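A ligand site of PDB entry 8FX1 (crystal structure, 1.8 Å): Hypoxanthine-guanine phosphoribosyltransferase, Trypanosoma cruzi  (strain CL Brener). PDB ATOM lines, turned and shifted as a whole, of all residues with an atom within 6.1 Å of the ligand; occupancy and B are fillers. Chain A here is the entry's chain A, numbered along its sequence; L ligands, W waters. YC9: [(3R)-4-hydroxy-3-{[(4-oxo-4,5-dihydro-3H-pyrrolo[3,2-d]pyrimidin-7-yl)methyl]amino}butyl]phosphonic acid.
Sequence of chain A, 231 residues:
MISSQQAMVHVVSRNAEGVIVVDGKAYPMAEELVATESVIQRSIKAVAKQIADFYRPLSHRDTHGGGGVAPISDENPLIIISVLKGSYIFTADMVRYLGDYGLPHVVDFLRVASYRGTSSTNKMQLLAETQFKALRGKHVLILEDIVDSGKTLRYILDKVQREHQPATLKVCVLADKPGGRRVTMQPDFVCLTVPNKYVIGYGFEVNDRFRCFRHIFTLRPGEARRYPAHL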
ATOM      1  N   VAL A  83      13.423 -34.082  -8.409  1.00  0.00           N
ATOM      2  CA  VAL A  83      12.209 -33.716  -7.618  1.00  0.00           C
ATOM      3  C   VAL A  83      11.734 -32.326  -8.058  1.00  0.00           C
ATOM      4  O   VAL A  83      12.359 -31.350  -7.707  1.00  0.00           O
ATOM      5  CB  VAL A  83      12.472 -33.801  -6.100  1.00  0.00           C
ATOM      6  CG1 VAL A  83      11.220 -33.420  -5.291  1.00  0.00           C
ATOM      7  CG2 VAL A  83      12.980 -35.199  -5.698  1.00  0.00           C
ATOM      8  N   LEU A  84      10.639 -32.264  -8.797  1.00  0.00           N
ATOM      9  CA  LEU A  84      10.058 -30.991  -9.272  1.00  0.00           C
ATOM     10  C   LEU A  84       9.403 -30.256  -8.102  1.00  0.00           C
ATOM     11  O   LEU A  84       9.003 -30.918  -7.163  1.00  0.00           O
ATOM     12  CB  LEU A  84       9.057 -31.286 -10.404  1.00  0.00           C
ATOM     13  CG  LEU A  84       9.662 -31.815 -11.704  1.00  0.00           C
ATOM     14  CD1 LEU A  84       8.554 -32.244 -12.679  1.00  0.00           C
ATOM     15  CD2 LEU A  84      10.585 -30.764 -12.346  1.00  0.00           C
ATOM     16  N   LYS A  85       9.260 -28.929  -8.200  1.00  0.00           N
ATOM     17  CA  LYS A  85       9.705 -28.066  -9.318  1.00  0.00           C
ATOM     18  C   LYS A  85      11.082 -27.487  -9.014  1.00  0.00           C
ATOM     19  O   LYS A  85      11.838 -27.247  -9.927  1.00  0.00           O
ATOM     20  CB  LYS A  85       8.693 -26.921  -9.585  1.00  0.00           C
ATOM     21  CG  LYS A  85       7.356 -27.357 -10.181  1.00  0.00           C
ATOM     22  CD  LYS A  85       6.535 -26.183 -10.789  1.00  0.00           C
ATOM     23  CE  LYS A  85       6.120 -25.133  -9.762  1.00  0.00           C
ATOM     24  NZ  LYS A  85       5.147 -24.136 -10.323  1.00  0.00           N
ATOM     25  N   GLY A  86      11.414 -27.329  -7.733  1.00  0.00           N
ATOM     26  CA  GLY A  86      12.641 -26.625  -7.324  1.00  0.00           C
ATOM     27  C   GLY A  86      13.949 -27.159  -7.911  1.00  0.00           C
ATOM     28  O   GLY A  86      14.878 -26.371  -8.003  1.00  0.00           O
ATOM     29  N   VAL A 112       6.319 -33.907  -5.084  1.00  0.00           N
ATOM     30  CA  VAL A 112       5.678 -34.171  -3.775  1.00  0.00           C
ATOM     31  C   VAL A 112       5.212 -32.833  -3.195  1.00  0.00           C
ATOM     32  O   VAL A 112       5.751 -31.808  -3.610  1.00  0.00           O
ATOM     33  CB  VAL A 112       6.607 -34.898  -2.768  1.00  0.00           C
ATOM     34  CG1 VAL A 112       6.948 -36.312  -3.261  1.00  0.00           C
ATOM     35  CG2 VAL A 112       7.893 -34.120  -2.462  1.00  0.00           C
ATOM     36  N   MET A 124       2.940 -35.554   3.946  1.00  0.00           N
ATOM     37  CA  MET A 124       3.370 -35.538   2.523  1.00  0.00           C
ATOM     38  C   MET A 124       2.376 -36.266   1.600  1.00  0.00           C
ATOM     39  O   MET A 124       1.736 -37.190   2.087  1.00  0.00           O
ATOM     40  CB  MET A 124       4.759 -36.195   2.369  1.00  0.00           C
ATOM     41  CG  MET A 124       5.898 -35.478   3.125  1.00  0.00           C
ATOM     42  SD  MET A 124       6.214 -33.796   2.556  1.00  0.00           S
ATOM     43  CE  MET A 124       6.264 -34.026   0.777  1.00  0.00           C
ATOM     44  N   GLU A 144      17.583 -33.363  -5.629  1.00  0.00           N
ATOM     45  CA  GLU A 144      16.681 -32.490  -4.857  1.00  0.00           C
ATOM     46  C   GLU A 144      17.348 -31.110  -4.661  1.00  0.00           C
ATOM     47  O   GLU A 144      18.536 -31.046  -4.624  1.00  0.00           O
ATOM     48  CB  GLU A 144      16.334 -33.155  -3.517  1.00  0.00           C
ATOM     49  CG  GLU A 144      15.415 -32.372  -2.589  1.00  0.00           C
ATOM     50  CD  GLU A 144      13.998 -32.195  -3.110  1.00  0.00           C
ATOM     51  OE1 GLU A 144      13.057 -32.726  -2.497  1.00  0.00           O
ATOM     52  OE2 GLU A 144      13.841 -31.508  -4.120  1.00  0.00           O
ATOM     53  N   ASP A 145      16.563 -30.056  -4.563  1.00  0.00           N
ATOM     54  CA  ASP A 145      17.089 -28.685  -4.413  1.00  0.00           C
ATOM     55  C   ASP A 145      17.647 -28.495  -2.986  1.00  0.00           C
ATOM     56  O   ASP A 145      18.749 -27.989  -2.860  1.00  0.00           O
ATOM     57  CB  ASP A 145      16.040 -27.620  -4.756  1.00  0.00           C
ATOM     58  CG  ASP A 145      14.731 -27.695  -3.997  1.00  0.00           C
ATOM     59  OD1 ASP A 145      14.526 -28.703  -3.352  1.00  0.00           O
ATOM     60  OD2 ASP A 145      13.932 -26.747  -4.069  1.00  0.00           O
ATOM     61  N   ILE A 146      16.898 -28.866  -1.968  1.00  0.00           N
ATOM     62  CA  ILE A 146      17.310 -28.589  -0.564  1.00  0.00           C
ATOM     63  C   ILE A 146      16.839 -29.656   0.412  1.00  0.00           C
ATOM     64  O   ILE A 146      15.780 -30.208   0.176  1.00  0.00           O
ATOM     65  CB  ILE A 146      16.811 -27.192  -0.102  1.00  0.00           C
ATOM     66  CG1 ILE A 146      17.421 -26.772   1.245  1.00  0.00           C
ATOM     67  CG2 ILE A 146      15.285 -27.103  -0.084  1.00  0.00           C
ATOM     68  CD1 ILE A 146      17.371 -25.263   1.518  1.00  0.00           C
ATOM     69  N   VAL A 147      17.648 -29.951   1.426  1.00  0.00           N
ATOM     70  CA  VAL A 147      17.271 -30.819   2.567  1.00  0.00           C
ATOM     71  C   VAL A 147      17.251 -29.836   3.741  1.00  0.00           C
ATOM     72  O   VAL A 147      18.254 -29.176   3.961  1.00  0.00           O
ATOM     73  CB  VAL A 147      18.223 -32.009   2.803  1.00  0.00           C
ATOM     74  CG1 VAL A 147      19.691 -31.596   2.992  1.00  0.00           C
ATOM     75  CG2 VAL A 147      17.741 -32.881   3.973  1.00  0.00           C
ATOM     76  N   ASP A 148      16.122 -29.699   4.431  1.00  0.00           N
ATOM     77  CA  ASP A 148      15.943 -28.757   5.567  1.00  0.00           C
ATOM     78  C   ASP A 148      15.506 -29.628   6.763  1.00  0.00           C
ATOM     79  O   ASP A 148      16.366 -30.074   7.487  1.00  0.00           O
ATOM     80  CB  ASP A 148      15.012 -27.639   5.074  1.00  0.00           C
ATOM     81  CG  ASP A 148      14.673 -26.518   6.046  1.00  0.00           C
ATOM     82  OD1 ASP A 148      14.799 -26.721   7.248  1.00  0.00           O
ATOM     83  OD2 ASP A 148      14.269 -25.441   5.576  1.00  0.00           O
ATOM     84  N   SER A 149      14.207 -29.918   6.909  1.00  0.00           N
ATOM     85  CA  SER A 149      13.666 -30.825   7.956  1.00  0.00           C
ATOM     86  C   SER A 149      14.067 -32.269   7.685  1.00  0.00           C
ATOM     87  O   SER A 149      14.200 -33.016   8.633  1.00  0.00           O
ATOM     88  CB  SER A 149      12.145 -30.731   8.081  1.00  0.00           C
ATOM     89  OG  SER A 149      11.475 -31.329   6.985  1.00  0.00           O
ATOM     90  N   GLY A 150      14.162 -32.653   6.412  1.00  0.00           N
ATOM     91  CA  GLY A 150      14.446 -34.047   5.995  1.00  0.00           C
ATOM     92  C   GLY A 150      13.173 -34.828   5.695  1.00  0.00           C
ATOM     93  O   GLY A 150      13.294 -35.959   5.243  1.00  0.00           O
ATOM     94  N   LYS A 151      11.996 -34.257   5.918  1.00  0.00           N
ATOM     95  CA  LYS A 151      10.695 -34.988   5.812  1.00  0.00           C
ATOM     96  C   LYS A 151      10.378 -35.377   4.358  1.00  0.00           C
ATOM     97  O   LYS A 151       9.963 -36.503   4.131  1.00  0.00           O
ATOM     98  CB  LYS A 151       9.561 -34.156   6.431  1.00  0.00           C
ATOM     99  CG  LYS A 151       9.657 -33.934   7.944  1.00  0.00           C
ATOM    100  CD  LYS A 151       9.270 -35.182   8.777  1.00  0.00           C
ATOM    101  CE  LYS A 151       7.775 -35.499   8.754  1.00  0.00           C
ATOM    102  NZ  LYS A 151       7.433 -36.698   9.585  1.00  0.00           N
ATOM    103  N   THR A 152      10.580 -34.466   3.414  1.00  0.00           N
ATOM    104  CA  THR A 152      10.238 -34.760   1.991  1.00  0.00           C
ATOM    105  C   THR A 152      11.115 -35.921   1.509  1.00  0.00           C
ATOM    106  O   THR A 152      10.583 -36.827   0.903  1.00  0.00           O
ATOM    107  CB  THR A 152      10.378 -33.531   1.077  1.00  0.00           C
ATOM    108  OG1 THR A 152      11.735 -33.169   1.239  1.00  0.00           O
ATOM    109  CG2 THR A 152       9.416 -32.405   1.388  1.00  0.00           C
ATOM    110  N   LEU A 153      12.407 -35.910   1.800  1.00  0.00           N
ATOM    111  CA  LEU A 153      13.333 -36.935   1.252  1.00  0.00           C
ATOM    112  C   LEU A 153      13.125 -38.268   1.993  1.00  0.00           C
ATOM    113  O   LEU A 153      13.262 -39.285   1.350  1.00  0.00           O
ATOM    114  CB  LEU A 153      14.791 -36.437   1.323  1.00  0.00           C
ATOM    115  CG  LEU A 153      15.253 -35.542   0.168  1.00  0.00           C
ATOM    116  CD1 LEU A 153      16.587 -34.846   0.519  1.00  0.00           C
ATOM    117  CD2 LEU A 153      15.387 -36.351  -1.141  1.00  0.00           C
ATOM    118  N   LYS A 177      20.492 -27.340   4.502  1.00  0.00           N
ATOM    119  CA  LYS A 177      20.232 -26.414   5.629  1.00  0.00           C
ATOM    120  C   LYS A 177      20.353 -27.321   6.853  1.00  0.00           C
ATOM    121  O   LYS A 177      19.369 -27.885   7.277  1.00  0.00           O
ATOM    122  CB  LYS A 177      18.876 -25.696   5.534  1.00  0.00           C
ATOM    123  CG  LYS A 177      18.674 -24.559   6.545  1.00  0.00           C
ATOM    124  CD  LYS A 177      17.257 -23.968   6.532  1.00  0.00           C
ATOM    125  CE  LYS A 177      16.800 -23.517   5.138  1.00  0.00           C
ATOM    126  NZ  LYS A 177      15.473 -22.816   5.203  1.00  0.00           N
ATOM    127  N   LYS A 197      18.157 -20.057   7.350  1.00  0.00           N
ATOM    128  CA  LYS A 197      17.279 -18.944   6.945  1.00  0.00           C
ATOM    129  C   LYS A 197      16.546 -19.370   5.664  1.00  0.00           C
ATOM    130  O   LYS A 197      17.007 -20.303   5.024  1.00  0.00           O
ATOM    131  CB  LYS A 197      18.109 -17.678   6.673  1.00  0.00           C
ATOM    132  CG  LYS A 197      18.982 -17.145   7.817  1.00  0.00           C
ATOM    133  CD  LYS A 197      18.230 -16.251   8.819  1.00  0.00           C
ATOM    134  CE  LYS A 197      19.138 -15.561   9.833  1.00  0.00           C
ATOM    135  NZ  LYS A 197      18.631 -14.210  10.225  1.00  0.00           N
ATOM    136  N   TYR A 198      15.458 -18.694   5.299  1.00  0.00           N
ATOM    137  CA  TYR A 198      14.728 -18.960   4.040  1.00  0.00           C
ATOM    138  C   TYR A 198      15.605 -18.478   2.878  1.00  0.00           C
ATOM    139  O   TYR A 198      15.880 -17.291   2.847  1.00  0.00           O
ATOM    140  CB  TYR A 198      13.355 -18.297   4.003  1.00  0.00           C
ATOM    141  CG  TYR A 198      12.427 -18.840   2.948  1.00  0.00           C
ATOM    142  CD1 TYR A 198      11.642 -19.951   3.218  1.00  0.00           C
ATOM    143  CD2 TYR A 198      12.349 -18.287   1.682  1.00  0.00           C
ATOM    144  CE1 TYR A 198      10.795 -20.489   2.263  1.00  0.00           C
ATOM    145  CE2 TYR A 198      11.494 -18.805   0.722  1.00  0.00           C
ATOM    146  CZ  TYR A 198      10.706 -19.904   1.020  1.00  0.00           C
ATOM    147  OH  TYR A 198       9.864 -20.472   0.108  1.00  0.00           O
ATOM    148  N   VAL A 199      16.018 -19.367   1.981  1.00  0.00           N
ATOM    149  CA  VAL A 199      16.921 -19.027   0.830  1.00  0.00           C
ATOM    150  C   VAL A 199      16.068 -18.694  -0.421  1.00  0.00           C
ATOM    151  O   VAL A 199      14.967 -18.974  -0.474  1.00  0.00           O
ATOM    152  CB  VAL A 199      17.953 -20.158   0.570  1.00  0.00           C
ATOM    153  CG1 VAL A 199      18.958 -20.243   1.726  1.00  0.00           C
ATOM    154  CG2 VAL A 199      17.334 -21.539   0.293  1.00  0.00           C
ATOM    155  N   ILE A 200      16.553 -17.951  -1.366  1.00  0.00           N
ATOM    156  CA  ILE A 200      15.810 -17.674  -2.619  1.00  0.00           C
ATOM    157  C   ILE A 200      16.827 -17.693  -3.747  1.00  0.00           C
ATOM    158  O   ILE A 200      17.978 -17.518  -3.450  1.00  0.00           O
ATOM    159  CB  ILE A 200      15.009 -16.350  -2.560  1.00  0.00           C
ATOM    160  CG1 ILE A 200      15.892 -15.167  -2.127  1.00  0.00           C
ATOM    161  CG2 ILE A 200      13.756 -16.484  -1.664  1.00  0.00           C
ATOM    162  CD1 ILE A 200      15.320 -13.795  -2.525  1.00  0.00           C
ATOM    163  N   PHE A 204      15.036 -21.720  -5.852  1.00  0.00           N
ATOM    164  CA  PHE A 204      14.393 -21.420  -4.552  1.00  0.00           C
ATOM    165  C   PHE A 204      13.451 -20.219  -4.753  1.00  0.00           C
ATOM    166  O   PHE A 204      13.843 -19.310  -5.448  1.00  0.00           O
ATOM    167  CB  PHE A 204      15.443 -21.226  -3.453  1.00  0.00           C
ATOM    168  CG  PHE A 204      16.325 -22.429  -3.213  1.00  0.00           C
ATOM    169  CD1 PHE A 204      15.762 -23.651  -2.890  1.00  0.00           C
ATOM    170  CD2 PHE A 204      17.696 -22.333  -3.302  1.00  0.00           C
ATOM    171  CE1 PHE A 204      16.559 -24.758  -2.677  1.00  0.00           C
ATOM    172  CE2 PHE A 204      18.497 -23.446  -3.083  1.00  0.00           C
ATOM    173  CZ  PHE A 204      17.927 -24.655  -2.774  1.00  0.00           C
ATOM    174  N   GLU A 205      12.284 -20.217  -4.131  1.00  0.00           N
ATOM    175  CA  GLU A 205      11.269 -19.178  -4.441  1.00  0.00           C
ATOM    176  C   GLU A 205      10.327 -18.785  -3.323  1.00  0.00           C
ATOM    177  O   GLU A 205      10.370 -19.403  -2.297  1.00  0.00           O
ATOM    178  CB  GLU A 205      10.364 -19.733  -5.548  1.00  0.00           C
ATOM    179  CG  GLU A 205       9.840 -21.156  -5.350  1.00  0.00           C
ATOM    180  CD  GLU A 205       8.864 -21.395  -4.200  1.00  0.00           C
ATOM    181  OE1 GLU A 205       9.148 -22.208  -3.314  1.00  0.00           O
ATOM    182  OE2 GLU A 205       7.781 -20.777  -4.211  1.00  0.00           O
HETATM  183  C10 YC9 L   1      12.172 -29.531   1.005  1.00  0.00           C
HETATM  184  C01 YC9 L   1      13.918 -22.570   1.545  1.00  0.00           C
HETATM  185  C02 YC9 L   1      13.321 -23.928   1.691  1.00  0.00           C
HETATM  186  C03 YC9 L   1      12.461 -24.327   0.732  1.00  0.00           C
HETATM  187  C04 YC9 L   1      12.062 -25.599   1.106  1.00  0.00           C
HETATM  188  C05 YC9 L   1      12.739 -25.886   2.292  1.00  0.00           C
HETATM  189  C07 YC9 L   1      11.103 -26.471   0.320  1.00  0.00           C
HETATM  190  C09 YC9 L   1      11.531 -28.892  -0.253  1.00  0.00           C
HETATM  191  C11 YC9 L   1      11.346 -29.318   2.275  1.00  0.00           C
HETATM  192  C16 YC9 L   1      11.924 -29.667  -1.531  1.00  0.00           C
HETATM  193  C19 YC9 L   1      12.729 -22.111  -0.516  1.00  0.00           C
HETATM  194  N06 YC9 L   1      13.481 -24.854   2.614  1.00  0.00           N
HETATM  195  N08 YC9 L   1      11.952 -27.485  -0.315  1.00  0.00           N
HETATM  196  N18 YC9 L   1      12.135 -23.429  -0.391  1.00  0.00           N
HETATM  197  N20 YC9 L   1      13.646 -21.684   0.488  1.00  0.00           N
HETATM  198  O13 YC9 L   1      11.241 -31.413   4.051  1.00  0.00           O
HETATM  199  O14 YC9 L   1      11.915 -29.275   4.835  1.00  0.00           O
HETATM  200  O15 YC9 L   1      13.357 -30.816   3.469  1.00  0.00           O
HETATM  201  O17 YC9 L   1      11.568 -28.851  -2.631  1.00  0.00           O
HETATM  202  O21 YC9 L   1      14.634 -22.246   2.337  1.00  0.00           O
HETATM  203  P12 YC9 L   1      12.040 -30.240   3.717  1.00  0.00           P
HETATM  204  O   HOH W   1       8.648 -30.587   4.491  1.00  0.00           O
HETATM  205  O   HOH W   2      11.784 -23.044  -3.077  1.00  0.00           O
HETATM  206  O   HOH W   3      12.152 -29.719  -5.371  1.00  0.00           O
HETATM  207  O   HOH W   4      14.037 -33.470   2.684  1.00  0.00           O
HETATM  208  O   HOH W   5      13.950 -32.088   0.242  1.00  0.00           O
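The backbone NH (N) of Asp 148 lies within hydrogen-bond range of an oxygen (O15) of the ligand (3.1 Å). The backbone NH (N) of Ser 149 is in hydrogen-bond range of an oxygen (O14) of the ligand. An oxygen (O13) of the ligand is in hydrogen-bond range of the backbone NH (N) of Lys 151 (3.5 Å). An oxygen (O13) of the ligand is in hydrogen-bond range of the side-chain hydroxyl (OG1) of Thr 152. The side-chain amino group (NZ) of Lys 177 sits at hydrogen-bond distance from an oxygen (O21) of the ligand (3.0 Å). The backbone NH (N) of Thr 152 is in hydrogen-bond range of an oxygen (O13) of the ligand (3.2 Å). The backbone carbonyl oxygen (O) of Val 199 sits at hydrogen-bond distance from a nitrogen (N20) of the ligand (3.2 Å). N of Val 199 is in hydrogen-bond range of O21 of the ligand. A nitrogen (N06) of the ligand lies within hydrogen-bond range of the side-chain carboxylate (OD2) of Asp 148 (3.1 Å). O13 of the ligand is in hydrogen-bond range of OG of Ser 149, 2.9 Å away. The side-chain carboxylate of Asp 145 sits at hydrogen-bond distance from an oxygen (O17) of the ligand, at 3.0 Å.
The backbone NH of Lys 177 sits at hydrogen-bond distance from the backbone carbonyl oxygen of Val 147, 2.9 Å away. The side-chain hydroxyl of Tyr 198 lies within hydrogen-bond range of the backbone carbonyl oxygen of Glu 205 (2.7 Å). The side-chain amino group (NZ) of Lys 177 lies within hydrogen-bond range of the backbone carbonyl oxygen (O) of Lys 197. The side-chain hydroxyl (OG) of Ser 149 lies within hydrogen-bond range of the backbone NH (N) of Lys 151 (3.2 Å). NZ of Lys 177 lies within salt-bridge range of OD2 of Asp 148, at 2.9 Å.
OE1 of Glu 144 touches C16 of the ligand, at 3.4 Å. CG2 of Ile 146 touches N08 of the ligand, 3.4 Å away. Gly 150 touches the ligand (N to O15, 3.6 Å). Tyr 198 touches the ligand. 11 residues have an atom within 4 Å of the ligand: Glu 144, Asp 145, Ile 146, Asp 148, Ser 149, Gly 150, Lys 151, Thr 152, Lys 177, Tyr 198 and Val 199.
Water W2 lies within hydrogen-bond range of N18 of the ligand and OE1 of Glu 205. Water W4 lies within hydrogen-bond range of OG1 of Thr 152, O15 of the ligand and N of Leu 153. Water W5 lies within hydrogen-bond range of O of Ile 146, OG1 of Thr 152 and OE1 of Glu 144.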
